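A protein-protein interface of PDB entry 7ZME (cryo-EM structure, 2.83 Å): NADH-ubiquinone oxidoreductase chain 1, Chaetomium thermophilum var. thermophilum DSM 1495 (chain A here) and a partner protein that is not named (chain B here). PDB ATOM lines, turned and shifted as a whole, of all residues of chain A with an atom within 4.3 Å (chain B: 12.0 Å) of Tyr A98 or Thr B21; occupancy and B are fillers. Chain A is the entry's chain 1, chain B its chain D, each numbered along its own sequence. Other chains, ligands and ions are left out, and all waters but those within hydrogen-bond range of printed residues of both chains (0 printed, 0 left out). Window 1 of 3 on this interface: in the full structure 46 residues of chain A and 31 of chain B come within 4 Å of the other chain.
The backbone carbonyl oxygen of Leu A15 sits at hydrogen-bond distance from the side-chain hydroxyl of Thr B21, 2.9 Å away.
Among the printed residues, pairs that only touch across the chains: Leu A15 with Gly B24 (3.4 Å), Leu A15 with Met B25 (3.7 Å), Leu A15 with Val B28 (3.98 Å), Val A16 with Met B25 (3.9 Å), Pro A19 with Met B17 (3.5 Å), Pro A19 with Thr B21 (3.2 Å), Tyr A98 with Phe B18 (3.7 Å), Tyr A98 with Thr B21 (3.7 Å), Tyr A98 with Gly B22 (3.9 Å), Leu A102 with Met B25 (3.7 Å), Leu A102 with Ala B26 (3.8 Å), Leu A102 with Arg B29 (3.6 Å), Leu A102 with His B38 (3.6 Å) and Leu A316 with Phe B18 (3.8 Å).
The side-chain hydroxyl (OG) of Ser A20 is in hydrogen-bond range of the backbone carbonyl oxygen (O) of Val A16.
The side-chain hydroxyl (OG1) of Thr B21 sits at hydrogen-bond distance from the backbone carbonyl oxygen (O) of Met B17 (3.1 Å).
Of chain B, only Phe B18, Thr B21 and Gly B22 come within 4 Å of Tyr A98.
Of the printed residues of chain B, Leu A15 touches Thr B21 (2.9 Å), Gly B24 (3.4 Å), Met B25 (3.7 Å) and Val B28 (3.98 Å).
Val A16 touches just one residue of chain B: Met B25 (3.9 Å).
Pro A19 touches just these residues of chain B: Met B17 (3.5 Å) and Thr B21 (3.2 Å).
No residue of chain B comes within 4 Å of Ser A20.
No residue of chain B comes within 4 Å of Tyr A93.
No residue of chain B comes within 4 Å of Ile A96.
Pro A97 touches none of the printed residues of chain B.
No residue of chain B comes within 4 Å of Gly A99.
Leu A102 touches four residues of chain B.
Of the printed residues of chain A, Val B28 touches Leu A15.
Of the printed residues of chain A, Phe B18 touches Tyr A98 (3.7 Å) and Leu A316 (3.8 Å).
Of the printed residues of chain A, Met B25 touches Leu A15, Val A16 and Leu A102.
Tyr A312 touches none of the printed residues of chain B.
Gly B12 touches none of the printed residues of chain A.
The nearest printed residue of chain A that does not touch Met B25 is Tyr A98 (5.3 Å).
Of the 24 printed residues of chain B, 10 touch a printed residue of chain A.
Hydrophobic or aromatic side chains of chain B that line the printed part of chain A: Met B17, Phe B18, Met B25, Ala B26, Val B28 and His B38.
Printed residues of chain A that touch a printed residue of chain B: Leu A15, Val A16, Pro A19, Tyr A98, Leu A102 and Leu A316.
Hydrophobic or aromatic side chains of chain A that line the printed part of chain B: Leu A15, Val A16, Pro A19, Tyr A98, Leu A102 and Leu A316.
Among the printed residues, 15 pairs touch across the chains.
Among the printed residues, no Asp or Glu carboxylate lies within 4 Å of a Lys or Arg side-chain nitrogen of the other chain.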
ATOM      1  N   LEU A  15       0.254  16.718  12.973  1.00  0.00           N
ATOM      2  CA  LEU A  15       0.756  15.350  13.014  1.00  0.00           C
ATOM      3  C   LEU A  15       2.090  15.189  12.298  1.00  0.00           C
ATOM      4  O   LEU A  15       2.755  14.168  12.484  1.00  0.00           O
ATOM      5  CB  LEU A  15      -0.268  14.399  12.402  1.00  0.00           C
ATOM      6  CG  LEU A  15      -1.456  14.040  13.286  1.00  0.00           C
ATOM      7  CD1 LEU A  15      -2.565  13.433  12.446  1.00  0.00           C
ATOM      8  CD2 LEU A  15      -1.025  13.092  14.383  1.00  0.00           C
ATOM      9  N   VAL A  16       2.493  16.160  11.481  1.00  0.00           N
ATOM     10  CA  VAL A  16       3.783  16.106  10.806  1.00  0.00           C
ATOM     11  C   VAL A  16       4.790  16.966  11.556  1.00  0.00           C
ATOM     12  O   VAL A  16       5.855  16.484  11.953  1.00  0.00           O
ATOM     13  CB  VAL A  16       3.676  16.550   9.335  1.00  0.00           C
ATOM     14  CG1 VAL A  16       5.050  16.583   8.693  1.00  0.00           C
ATOM     15  CG2 VAL A  16       2.765  15.625   8.563  1.00  0.00           C
ATOM     16  N   PRO A  19       5.588  15.966  15.611  1.00  0.00           N
ATOM     17  CA  PRO A  19       6.450  14.778  15.711  1.00  0.00           C
ATOM     18  C   PRO A  19       7.803  14.938  15.044  1.00  0.00           C
ATOM     19  O   PRO A  19       8.781  14.337  15.502  1.00  0.00           O
ATOM     20  CB  PRO A  19       5.605  13.691  15.039  1.00  0.00           C
ATOM     21  CG  PRO A  19       4.230  14.114  15.310  1.00  0.00           C
ATOM     22  CD  PRO A  19       4.262  15.590  15.089  1.00  0.00           C
ATOM     23  N   SER A  20       7.892  15.720  13.968  1.00  0.00           N
ATOM     24  CA  SER A  20       9.192  15.942  13.350  1.00  0.00           C
ATOM     25  C   SER A  20      10.076  16.830  14.212  1.00  0.00           C
ATOM     26  O   SER A  20      11.292  16.627  14.261  1.00  0.00           O
ATOM     27  CB  SER A  20       9.028  16.550  11.959  1.00  0.00           C
ATOM     28  OG  SER A  20       8.328  15.672  11.099  1.00  0.00           O
ATOM     29  N   TYR A  93       9.371  19.145   4.751  1.00  0.00           N
ATOM     30  CA  TYR A  93       8.615  18.042   5.330  1.00  0.00           C
ATOM     31  C   TYR A  93       7.164  18.061   4.876  1.00  0.00           C
ATOM     32  O   TYR A  93       6.343  17.297   5.392  1.00  0.00           O
ATOM     33  CB  TYR A  93       8.666  18.087   6.859  1.00  0.00           C
ATOM     34  CG  TYR A  93      10.020  17.802   7.467  1.00  0.00           C
ATOM     35  CD1 TYR A  93      11.052  18.722   7.378  1.00  0.00           C
ATOM     36  CD2 TYR A  93      10.257  16.619   8.144  1.00  0.00           C
ATOM     37  CE1 TYR A  93      12.280  18.467   7.937  1.00  0.00           C
ATOM     38  CE2 TYR A  93      11.485  16.353   8.705  1.00  0.00           C
ATOM     39  CZ  TYR A  93      12.492  17.278   8.600  1.00  0.00           C
ATOM     40  OH  TYR A  93      13.716  17.014   9.161  1.00  0.00           O
ATOM     41  N   ILE A  96       6.786  14.946   2.203  1.00  0.00           N
ATOM     42  CA  ILE A  96       7.238  13.597   2.655  1.00  0.00           C
ATOM     43  C   ILE A  96       6.057  12.620   2.734  1.00  0.00           C
ATOM     44  O   ILE A  96       5.165  12.873   3.547  1.00  0.00           O
ATOM     45  CB  ILE A  96       8.046  13.656   3.960  1.00  0.00           C
ATOM     46  CG1 ILE A  96       9.311  14.500   3.787  1.00  0.00           C
ATOM     47  CG2 ILE A  96       8.359  12.252   4.456  1.00  0.00           C
ATOM     48  CD1 ILE A  96      10.172  14.085   2.619  1.00  0.00           C
ATOM     49  N   PRO A  97       5.976  11.527   1.939  1.00  0.00           N
ATOM     50  CA  PRO A  97       4.893  10.552   2.118  1.00  0.00           C
ATOM     51  C   PRO A  97       5.207   9.599   3.265  1.00  0.00           C
ATOM     52  O   PRO A  97       6.202   8.874   3.232  1.00  0.00           O
ATOM     53  CB  PRO A  97       4.852   9.823   0.772  1.00  0.00           C
ATOM     54  CG  PRO A  97       6.252   9.903   0.272  1.00  0.00           C
ATOM     55  CD  PRO A  97       6.824  11.201   0.778  1.00  0.00           C
ATOM     56  N   TYR A  98       4.348   9.604   4.282  1.00  0.00           N
ATOM     57  CA  TYR A  98       4.399   8.633   5.367  1.00  0.00           C
ATOM     58  C   TYR A  98       3.489   7.443   5.100  1.00  0.00           C
ATOM     59  O   TYR A  98       2.914   6.867   6.031  1.00  0.00           O
ATOM     60  CB  TYR A  98       4.044   9.303   6.695  1.00  0.00           C
ATOM     61  CG  TYR A  98       4.980  10.426   7.076  1.00  0.00           C
ATOM     62  CD1 TYR A  98       4.803  11.704   6.569  1.00  0.00           C
ATOM     63  CD2 TYR A  98       6.048  10.205   7.932  1.00  0.00           C
ATOM     64  CE1 TYR A  98       5.654  12.730   6.908  1.00  0.00           C
ATOM     65  CE2 TYR A  98       6.909  11.226   8.275  1.00  0.00           C
ATOM     66  CZ  TYR A  98       6.705  12.488   7.761  1.00  0.00           C
ATOM     67  OH  TYR A  98       7.552  13.517   8.098  1.00  0.00           O
ATOM     68  N   GLY A  99       3.352   7.075   3.835  1.00  0.00           N
ATOM     69  CA  GLY A  99       2.343   6.169   3.357  1.00  0.00           C
ATOM     70  C   GLY A  99       1.927   6.651   1.987  1.00  0.00           C
ATOM     71  O   GLY A  99       2.306   7.744   1.565  1.00  0.00           O
ATOM     72  N   LEU A 102       0.155   9.992   1.888  1.00  0.00           N
ATOM     73  CA  LEU A 102      -0.019  10.512   3.271  1.00  0.00           C
ATOM     74  C   LEU A 102       0.983  11.641   3.491  1.00  0.00           C
ATOM     75  O   LEU A 102       1.906  11.461   4.281  1.00  0.00           O
ATOM     76  CB  LEU A 102       0.093   9.362   4.278  1.00  0.00           C
ATOM     77  CG  LEU A 102      -1.071   8.379   4.288  1.00  0.00           C
ATOM     78  CD1 LEU A 102      -0.800   7.251   5.263  1.00  0.00           C
ATOM     79  CD2 LEU A 102      -2.359   9.092   4.651  1.00  0.00           C
ATOM     80  N   TYR A 312       3.646   1.592   8.112  1.00  0.00           N
ATOM     81  CA  TYR A 312       4.298   2.428   7.106  1.00  0.00           C
ATOM     82  C   TYR A 312       5.213   3.459   7.754  1.00  0.00           C
ATOM     83  O   TYR A 312       6.341   3.668   7.300  1.00  0.00           O
ATOM     84  CB  TYR A 312       3.252   3.118   6.232  1.00  0.00           C
ATOM     85  CG  TYR A 312       2.725   2.264   5.107  1.00  0.00           C
ATOM     86  CD1 TYR A 312       3.500   1.256   4.550  1.00  0.00           C
ATOM     87  CD2 TYR A 312       1.450   2.461   4.601  1.00  0.00           C
ATOM     88  CE1 TYR A 312       3.022   0.478   3.525  1.00  0.00           C
ATOM     89  CE2 TYR A 312       0.962   1.684   3.577  1.00  0.00           C
ATOM     90  CZ  TYR A 312       1.750   0.699   3.039  1.00  0.00           C
ATOM     91  OH  TYR A 312       1.262  -0.075   2.012  1.00  0.00           O
ATOM     92  N   LEU A 316       9.483   3.504   7.382  1.00  0.00           N
ATOM     93  CA  LEU A 316      10.239   4.663   6.927  1.00  0.00           C
ATOM     94  C   LEU A 316      11.154   5.186   8.026  1.00  0.00           C
ATOM     95  O   LEU A 316      12.309   5.539   7.765  1.00  0.00           O
ATOM     96  CB  LEU A 316       9.284   5.756   6.453  1.00  0.00           C
ATOM     97  CG  LEU A 316       9.900   7.091   6.034  1.00  0.00           C
ATOM     98  CD1 LEU A 316      10.761   6.933   4.793  1.00  0.00           C
ATOM     99  CD2 LEU A 316       8.815   8.120   5.808  1.00  0.00           C
ATOM    100  N   GLY B  12      15.110   4.846  19.109  1.00  0.00           N
ATOM    101  CA  GLY B  12      13.774   4.292  19.241  1.00  0.00           C
ATOM    102  C   GLY B  12      12.701   5.363  19.281  1.00  0.00           C
ATOM    103  O   GLY B  12      11.596   5.163  18.775  1.00  0.00           O
ATOM    104  N   ILE B  13      13.010   6.509  19.892  1.00  0.00           N
ATOM    105  CA  ILE B  13      12.064   7.619  19.922  1.00  0.00           C
ATOM    106  C   ILE B  13      11.882   8.207  18.528  1.00  0.00           C
ATOM    107  O   ILE B  13      10.766   8.556  18.129  1.00  0.00           O
ATOM    108  CB  ILE B  13      12.525   8.683  20.936  1.00  0.00           C
ATOM    109  CG1 ILE B  13      12.310   8.184  22.367  1.00  0.00           C
ATOM    110  CG2 ILE B  13      11.800  10.000  20.710  1.00  0.00           C
ATOM    111  CD1 ILE B  13      13.062   8.975  23.412  1.00  0.00           C
ATOM    112  N   ILE B  14      12.970   8.320  17.763  1.00  0.00           N
ATOM    113  CA  ILE B  14      12.866   8.843  16.405  1.00  0.00           C
ATOM    114  C   ILE B  14      12.008   7.925  15.549  1.00  0.00           C
ATOM    115  O   ILE B  14      11.154   8.387  14.780  1.00  0.00           O
ATOM    116  CB  ILE B  14      14.267   9.038  15.796  1.00  0.00           C
ATOM    117  CG1 ILE B  14      15.033  10.133  16.539  1.00  0.00           C
ATOM    118  CG2 ILE B  14      14.164   9.404  14.326  1.00  0.00           C
ATOM    119  CD1 ILE B  14      16.529   9.973  16.461  1.00  0.00           C
ATOM    120  N   ILE B  15      12.217   6.612  15.666  1.00  0.00           N
ATOM    121  CA  ILE B  15      11.404   5.653  14.925  1.00  0.00           C
ATOM    122  C   ILE B  15       9.947   5.742  15.354  1.00  0.00           C
ATOM    123  O   ILE B  15       9.033   5.718  14.519  1.00  0.00           O
ATOM    124  CB  ILE B  15      11.957   4.228  15.111  1.00  0.00           C
ATOM    125  CG1 ILE B  15      13.333   4.095  14.466  1.00  0.00           C
ATOM    126  CG2 ILE B  15      10.998   3.205  14.535  1.00  0.00           C
ATOM    127  CD1 ILE B  15      14.003   2.774  14.726  1.00  0.00           C
ATOM    128  N   ALA B  16       9.703   5.844  16.661  1.00  0.00           N
ATOM    129  CA  ALA B  16       8.337   5.847  17.165  1.00  0.00           C
ATOM    130  C   ALA B  16       7.555   7.054  16.680  1.00  0.00           C
ATOM    131  O   ALA B  16       6.371   6.931  16.353  1.00  0.00           O
ATOM    132  CB  ALA B  16       8.340   5.804  18.691  1.00  0.00           C
ATOM    133  N   MET B  17       8.186   8.223  16.624  1.00  0.00           N
ATOM    134  CA  MET B  17       7.464   9.421  16.227  1.00  0.00           C
ATOM    135  C   MET B  17       7.147   9.422  14.740  1.00  0.00           C
ATOM    136  O   MET B  17       6.160  10.039  14.331  1.00  0.00           O
ATOM    137  CB  MET B  17       8.268  10.664  16.601  1.00  0.00           C
ATOM    138  CG  MET B  17       8.431  10.831  18.096  1.00  0.00           C
ATOM    139  SD  MET B  17       6.890  11.005  19.004  1.00  0.00           S
ATOM    140  CE  MET B  17       6.353  12.612  18.461  1.00  0.00           C
ATOM    141  N   PHE B  18       7.967   8.749  13.930  1.00  0.00           N
ATOM    142  CA  PHE B  18       7.577   8.446  12.559  1.00  0.00           C
ATOM    143  C   PHE B  18       6.341   7.561  12.533  1.00  0.00           C
ATOM    144  O   PHE B  18       5.449   7.751  11.699  1.00  0.00           O
ATOM    145  CB  PHE B  18       8.728   7.762  11.826  1.00  0.00           C
ATOM    146  CG  PHE B  18       9.601   8.697  11.050  1.00  0.00           C
ATOM    147  CD1 PHE B  18      10.604   9.410  11.678  1.00  0.00           C
ATOM    148  CD2 PHE B  18       9.437   8.845   9.690  1.00  0.00           C
ATOM    149  CE1 PHE B  18      11.414  10.263  10.965  1.00  0.00           C
ATOM    150  CE2 PHE B  18      10.245   9.698   8.974  1.00  0.00           C
ATOM    151  CZ  PHE B  18      11.235  10.406   9.615  1.00  0.00           C
ATOM    152  N   GLY B  19       6.278   6.578  13.433  1.00  0.00           N
ATOM    153  CA  GLY B  19       5.099   5.735  13.520  1.00  0.00           C
ATOM    154  C   GLY B  19       3.876   6.498  13.981  1.00  0.00           C
ATOM    155  O   GLY B  19       2.761   6.227  13.534  1.00  0.00           O
ATOM    156  N   VAL B  20       4.067   7.455  14.890  1.00  0.00           N
ATOM    157  CA  VAL B  20       2.974   8.327  15.307  1.00  0.00           C
ATOM    158  C   VAL B  20       2.427   9.096  14.117  1.00  0.00           C
ATOM    159  O   VAL B  20       1.211   9.214  13.937  1.00  0.00           O
ATOM    160  CB  VAL B  20       3.445   9.279  16.421  1.00  0.00           C
ATOM    161  CG1 VAL B  20       2.348  10.261  16.782  1.00  0.00           C
ATOM    162  CG2 VAL B  20       3.874   8.494  17.644  1.00  0.00           C
ATOM    163  N   THR B  21       3.319   9.631  13.283  1.00  0.00           N
ATOM    164  CA  THR B  21       2.889  10.437  12.147  1.00  0.00           C
ATOM    165  C   THR B  21       2.143   9.589  11.127  1.00  0.00           C
ATOM    166  O   THR B  21       1.039   9.942  10.707  1.00  0.00           O
ATOM    167  CB  THR B  21       4.096  11.124  11.512  1.00  0.00           C
ATOM    168  OG1 THR B  21       4.663  12.041  12.452  1.00  0.00           O
ATOM    169  CG2 THR B  21       3.696  11.883  10.256  1.00  0.00           C
ATOM    170  N   GLY B  22       2.717   8.447  10.745  1.00  0.00           N
ATOM    171  CA  GLY B  22       2.070   7.597   9.759  1.00  0.00           C
ATOM    172  C   GLY B  22       0.720   7.087  10.218  1.00  0.00           C
ATOM    173  O   GLY B  22      -0.237   7.053   9.442  1.00  0.00           O
ATOM    174  N   ALA B  23       0.622   6.686  11.486  1.00  0.00           N
ATOM    175  CA  ALA B  23      -0.656   6.229  12.020  1.00  0.00           C
ATOM    176  C   ALA B  23      -1.668   7.364  12.085  1.00  0.00           C
ATOM    177  O   ALA B  23      -2.851   7.165  11.789  1.00  0.00           O
ATOM    178  CB  ALA B  23      -0.456   5.609  13.400  1.00  0.00           C
ATOM    179  N   GLY B  24      -1.280   8.563  12.488  1.00  0.00           N
ATOM    180  CA  GLY B  24      -2.317   9.599  12.669  1.00  0.00           C
ATOM    181  C   GLY B  24      -2.820  10.178  11.372  1.00  0.00           C
ATOM    182  O   GLY B  24      -4.024  10.356  11.261  1.00  0.00           O
ATOM    183  N   MET B  25      -1.936  10.393  10.406  1.00  0.00           N
ATOM    184  CA  MET B  25      -2.331  10.908   9.084  1.00  0.00           C
ATOM    185  C   MET B  25      -3.294   9.906   8.472  1.00  0.00           C
ATOM    186  O   MET B  25      -4.310  10.332   7.905  1.00  0.00           O
ATOM    187  CB  MET B  25      -1.113  10.978   8.163  1.00  0.00           C
ATOM    188  CG  MET B  25      -0.209  12.156   8.426  1.00  0.00           C
ATOM    189  SD  MET B  25      -0.937  13.689   7.822  1.00  0.00           S
ATOM    190  CE  MET B  25       0.038  13.950   6.344  1.00  0.00           C
ATOM    191  N   ALA B  26      -2.986   8.625   8.602  1.00  0.00           N
ATOM    192  CA  ALA B  26      -3.846   7.588   8.015  1.00  0.00           C
ATOM    193  C   ALA B  26      -5.233   7.607   8.667  1.00  0.00           C
ATOM    194  O   ALA B  26      -6.222   7.500   7.939  1.00  0.00           O
ATOM    195  CB  ALA B  26      -3.159   6.265   8.128  1.00  0.00           C
ATOM    196  N   LYS B  27      -5.305   7.733   9.985  1.00  0.00           N
ATOM    197  CA  LYS B  27      -6.613   7.689  10.673  1.00  0.00           C
ATOM    198  C   LYS B  27      -7.454   8.920  10.322  1.00  0.00           C
ATOM    199  O   LYS B  27      -8.652   8.758  10.060  1.00  0.00           O
ATOM    200  CB  LYS B  27      -6.378   7.569  12.178  1.00  0.00           C
ATOM    201  CG  LYS B  27      -7.627   7.464  13.040  1.00  0.00           C
ATOM    202  CD  LYS B  27      -8.439   6.219  12.762  1.00  0.00           C
ATOM    203  CE  LYS B  27      -9.551   6.013  13.768  1.00  0.00           C
ATOM    204  NZ  LYS B  27     -10.405   7.217  13.888  1.00  0.00           N
ATOM    205  N   VAL B  28      -6.843  10.105  10.334  1.00  0.00           N
ATOM    206  CA  VAL B  28      -7.611  11.353  10.087  1.00  0.00           C
ATOM    207  C   VAL B  28      -8.129  11.377   8.646  1.00  0.00           C
ATOM    208  O   VAL B  28      -9.259  11.813   8.448  1.00  0.00           O
ATOM    209  CB  VAL B  28      -6.831  12.609  10.517  1.00  0.00           C
ATOM    210  CG1 VAL B  28      -6.408  12.521  11.973  1.00  0.00           C
ATOM    211  CG2 VAL B  28      -5.636  12.897   9.629  1.00  0.00           C
ATOM    212  N   ARG B  29      -7.320  10.934   7.686  1.00  0.00           N
ATOM    213  CA  ARG B  29      -7.738  10.886   6.260  1.00  0.00           C
ATOM    214  C   ARG B  29      -8.836   9.845   6.075  1.00  0.00           C
ATOM    215  O   ARG B  29      -9.727  10.100   5.282  1.00  0.00           O
ATOM    216  CB  ARG B  29      -6.533  10.686   5.334  1.00  0.00           C
ATOM    217  CG  ARG B  29      -6.227  11.841   4.398  1.00  0.00           C
ATOM    218  CD  ARG B  29      -4.995  11.381   3.649  1.00  0.00           C
ATOM    219  NE  ARG B  29      -4.395  12.326   2.726  1.00  0.00           N
ATOM    220  CZ  ARG B  29      -3.341  13.070   3.009  1.00  0.00           C
ATOM    221  NH1 ARG B  29      -2.770  12.986   4.198  1.00  0.00           N
ATOM    222  NH2 ARG B  29      -2.860  13.899   2.105  1.00  0.00           N
ATOM    223  N   HIS B  30      -8.736   8.712   6.759  1.00  0.00           N
ATOM    224  CA  HIS B  30      -9.756   7.633   6.680  1.00  0.00           C
ATOM    225  C   HIS B  30     -11.087   8.186   7.181  1.00  0.00           C
ATOM    226  O   HIS B  30     -12.077   7.900   6.541  1.00  0.00           O
ATOM    227  CB  HIS B  30      -9.217   6.415   7.429  1.00  0.00           C
ATOM    228  CG  HIS B  30      -9.978   5.141   7.301  1.00  0.00           C
ATOM    229  ND1 HIS B  30     -10.910   4.744   8.236  1.00  0.00           N
ATOM    230  CD2 HIS B  30      -9.888   4.133   6.409  1.00  0.00           C
ATOM    231  CE1 HIS B  30     -11.391   3.567   7.900  1.00  0.00           C
ATOM    232  NE2 HIS B  30     -10.787   3.175   6.780  1.00  0.00           N
ATOM    233  N   ARG B  37     -10.239   4.139   2.655  1.00  0.00           N
ATOM    234  CA  ARG B  37      -8.853   4.569   2.419  1.00  0.00           C
ATOM    235  C   ARG B  37      -8.941   5.796   1.515  1.00  0.00           C
ATOM    236  O   ARG B  37      -9.859   5.854   0.692  1.00  0.00           O
ATOM    237  CB  ARG B  37      -7.967   3.416   1.949  1.00  0.00           C
ATOM    238  CG  ARG B  37      -6.515   3.795   1.704  1.00  0.00           C
ATOM    239  CD  ARG B  37      -5.516   2.687   1.991  1.00  0.00           C
ATOM    240  NE  ARG B  37      -5.842   1.421   1.357  1.00  0.00           N
ATOM    241  CZ  ARG B  37      -6.280   0.345   1.997  1.00  0.00           C
ATOM    242  NH1 ARG B  37      -6.559  -0.758   1.323  1.00  0.00           N
ATOM    243  NH2 ARG B  37      -6.436   0.369   3.307  1.00  0.00           N
ATOM    244  N   HIS B  38      -8.039   6.750   1.695  1.00  0.00           N
ATOM    245  CA  HIS B  38      -8.042   8.008   0.907  1.00  0.00           C
ATOM    246  C   HIS B  38      -7.557   7.716  -0.512  1.00  0.00           C
ATOM    247  O   HIS B  38      -7.168   6.583  -0.774  1.00  0.00           O
ATOM    248  CB  HIS B  38      -7.137   9.008   1.617  1.00  0.00           C
ATOM    249  CG  HIS B  38      -5.698   8.641   1.498  1.00  0.00           C
ATOM    250  ND1 HIS B  38      -5.150   7.569   2.174  1.00  0.00           N
ATOM    251  CD2 HIS B  38      -4.704   9.172   0.758  1.00  0.00           C
ATOM    252  CE1 HIS B  38      -3.881   7.458   1.860  1.00  0.00           C
ATOM    253  NE2 HIS B  38      -3.583   8.435   1.001  1.00  0.00           N
ATOM    254  N   ARG B  39      -7.651   8.688  -1.405  1.00  0.00           N
ATOM    255  CA  ARG B  39      -7.112   8.516  -2.772  1.00  0.00           C
ATOM    256  C   ARG B  39      -5.763   9.222  -2.903  1.00  0.00           C
ATOM    257  O   ARG B  39      -5.610  10.268  -2.301  1.00  0.00           O
ATOM    258  CB  ARG B  39      -8.107   9.096  -3.779  1.00  0.00           C
ATOM    259  CG  ARG B  39      -9.519   8.541  -3.688  1.00  0.00           C
ATOM    260  CD  ARG B  39      -9.602   7.125  -4.213  1.00  0.00           C
ATOM    261  NE  ARG B  39      -9.044   7.011  -5.549  1.00  0.00           N
ATOM    262  CZ  ARG B  39      -9.716   7.259  -6.663  1.00  0.00           C
ATOM    263  NH1 ARG B  39     -10.976   7.648  -6.597  1.00  0.00           N
ATOM    264  NH2 ARG B  39      -9.128   7.123  -7.836  1.00  0.00           N
ATOM    265  N   TRP B  40      -4.835   8.684  -3.691  1.00  0.00           N
ATOM    266  CA  TRP B  40      -3.519   9.322  -3.947  1.00  0.00           C
ATOM    267  C   TRP B  40      -3.210   9.329  -5.439  1.00  0.00           C
ATOM    268  O   TRP B  40      -3.919   8.639  -6.179  1.00  0.00           O
ATOM    269  CB  TRP B  40      -2.401   8.621  -3.166  1.00  0.00           C
ATOM    270  CG  TRP B  40      -2.191   7.161  -3.424  1.00  0.00           C
ATOM    271  CD1 TRP B  40      -1.301   6.602  -4.292  1.00  0.00           C
ATOM    272  CD2 TRP B  40      -2.838   6.065  -2.756  1.00  0.00           C
ATOM    273  NE1 TRP B  40      -1.370   5.238  -4.235  1.00  0.00           N
ATOM    274  CE2 TRP B  40      -2.305   4.877  -3.302  1.00  0.00           C
ATOM    275  CE3 TRP B  40      -3.824   5.968  -1.769  1.00  0.00           C
ATOM    276  CZ2 TRP B  40      -2.723   3.614  -2.888  1.00  0.00           C
ATOM    277  CZ3 TRP B  40      -4.238   4.720  -1.364  1.00  0.00           C
ATOM    278  CH2 TRP B  40      -3.692   3.562  -1.913  1.00  0.00           C
ATOM    279  N   SER B  41      -2.188  10.085  -5.851  1.00  0.00           N
ATOM    280  CA  SER B  41      -1.742  10.111  -7.265  1.00  0.00           C
ATOM    281  C   SER B  41      -2.947  10.384  -8.157  1.00  0.00           C
ATOM    282  O   SER B  41      -3.136   9.647  -9.130  1.00  0.00           O
ATOM    283  CB  SER B  41      -1.011   8.856  -7.607  1.00  0.00           C
ATOM    284  OG  SER B  41       0.135   8.710  -6.785  1.00  0.00           O
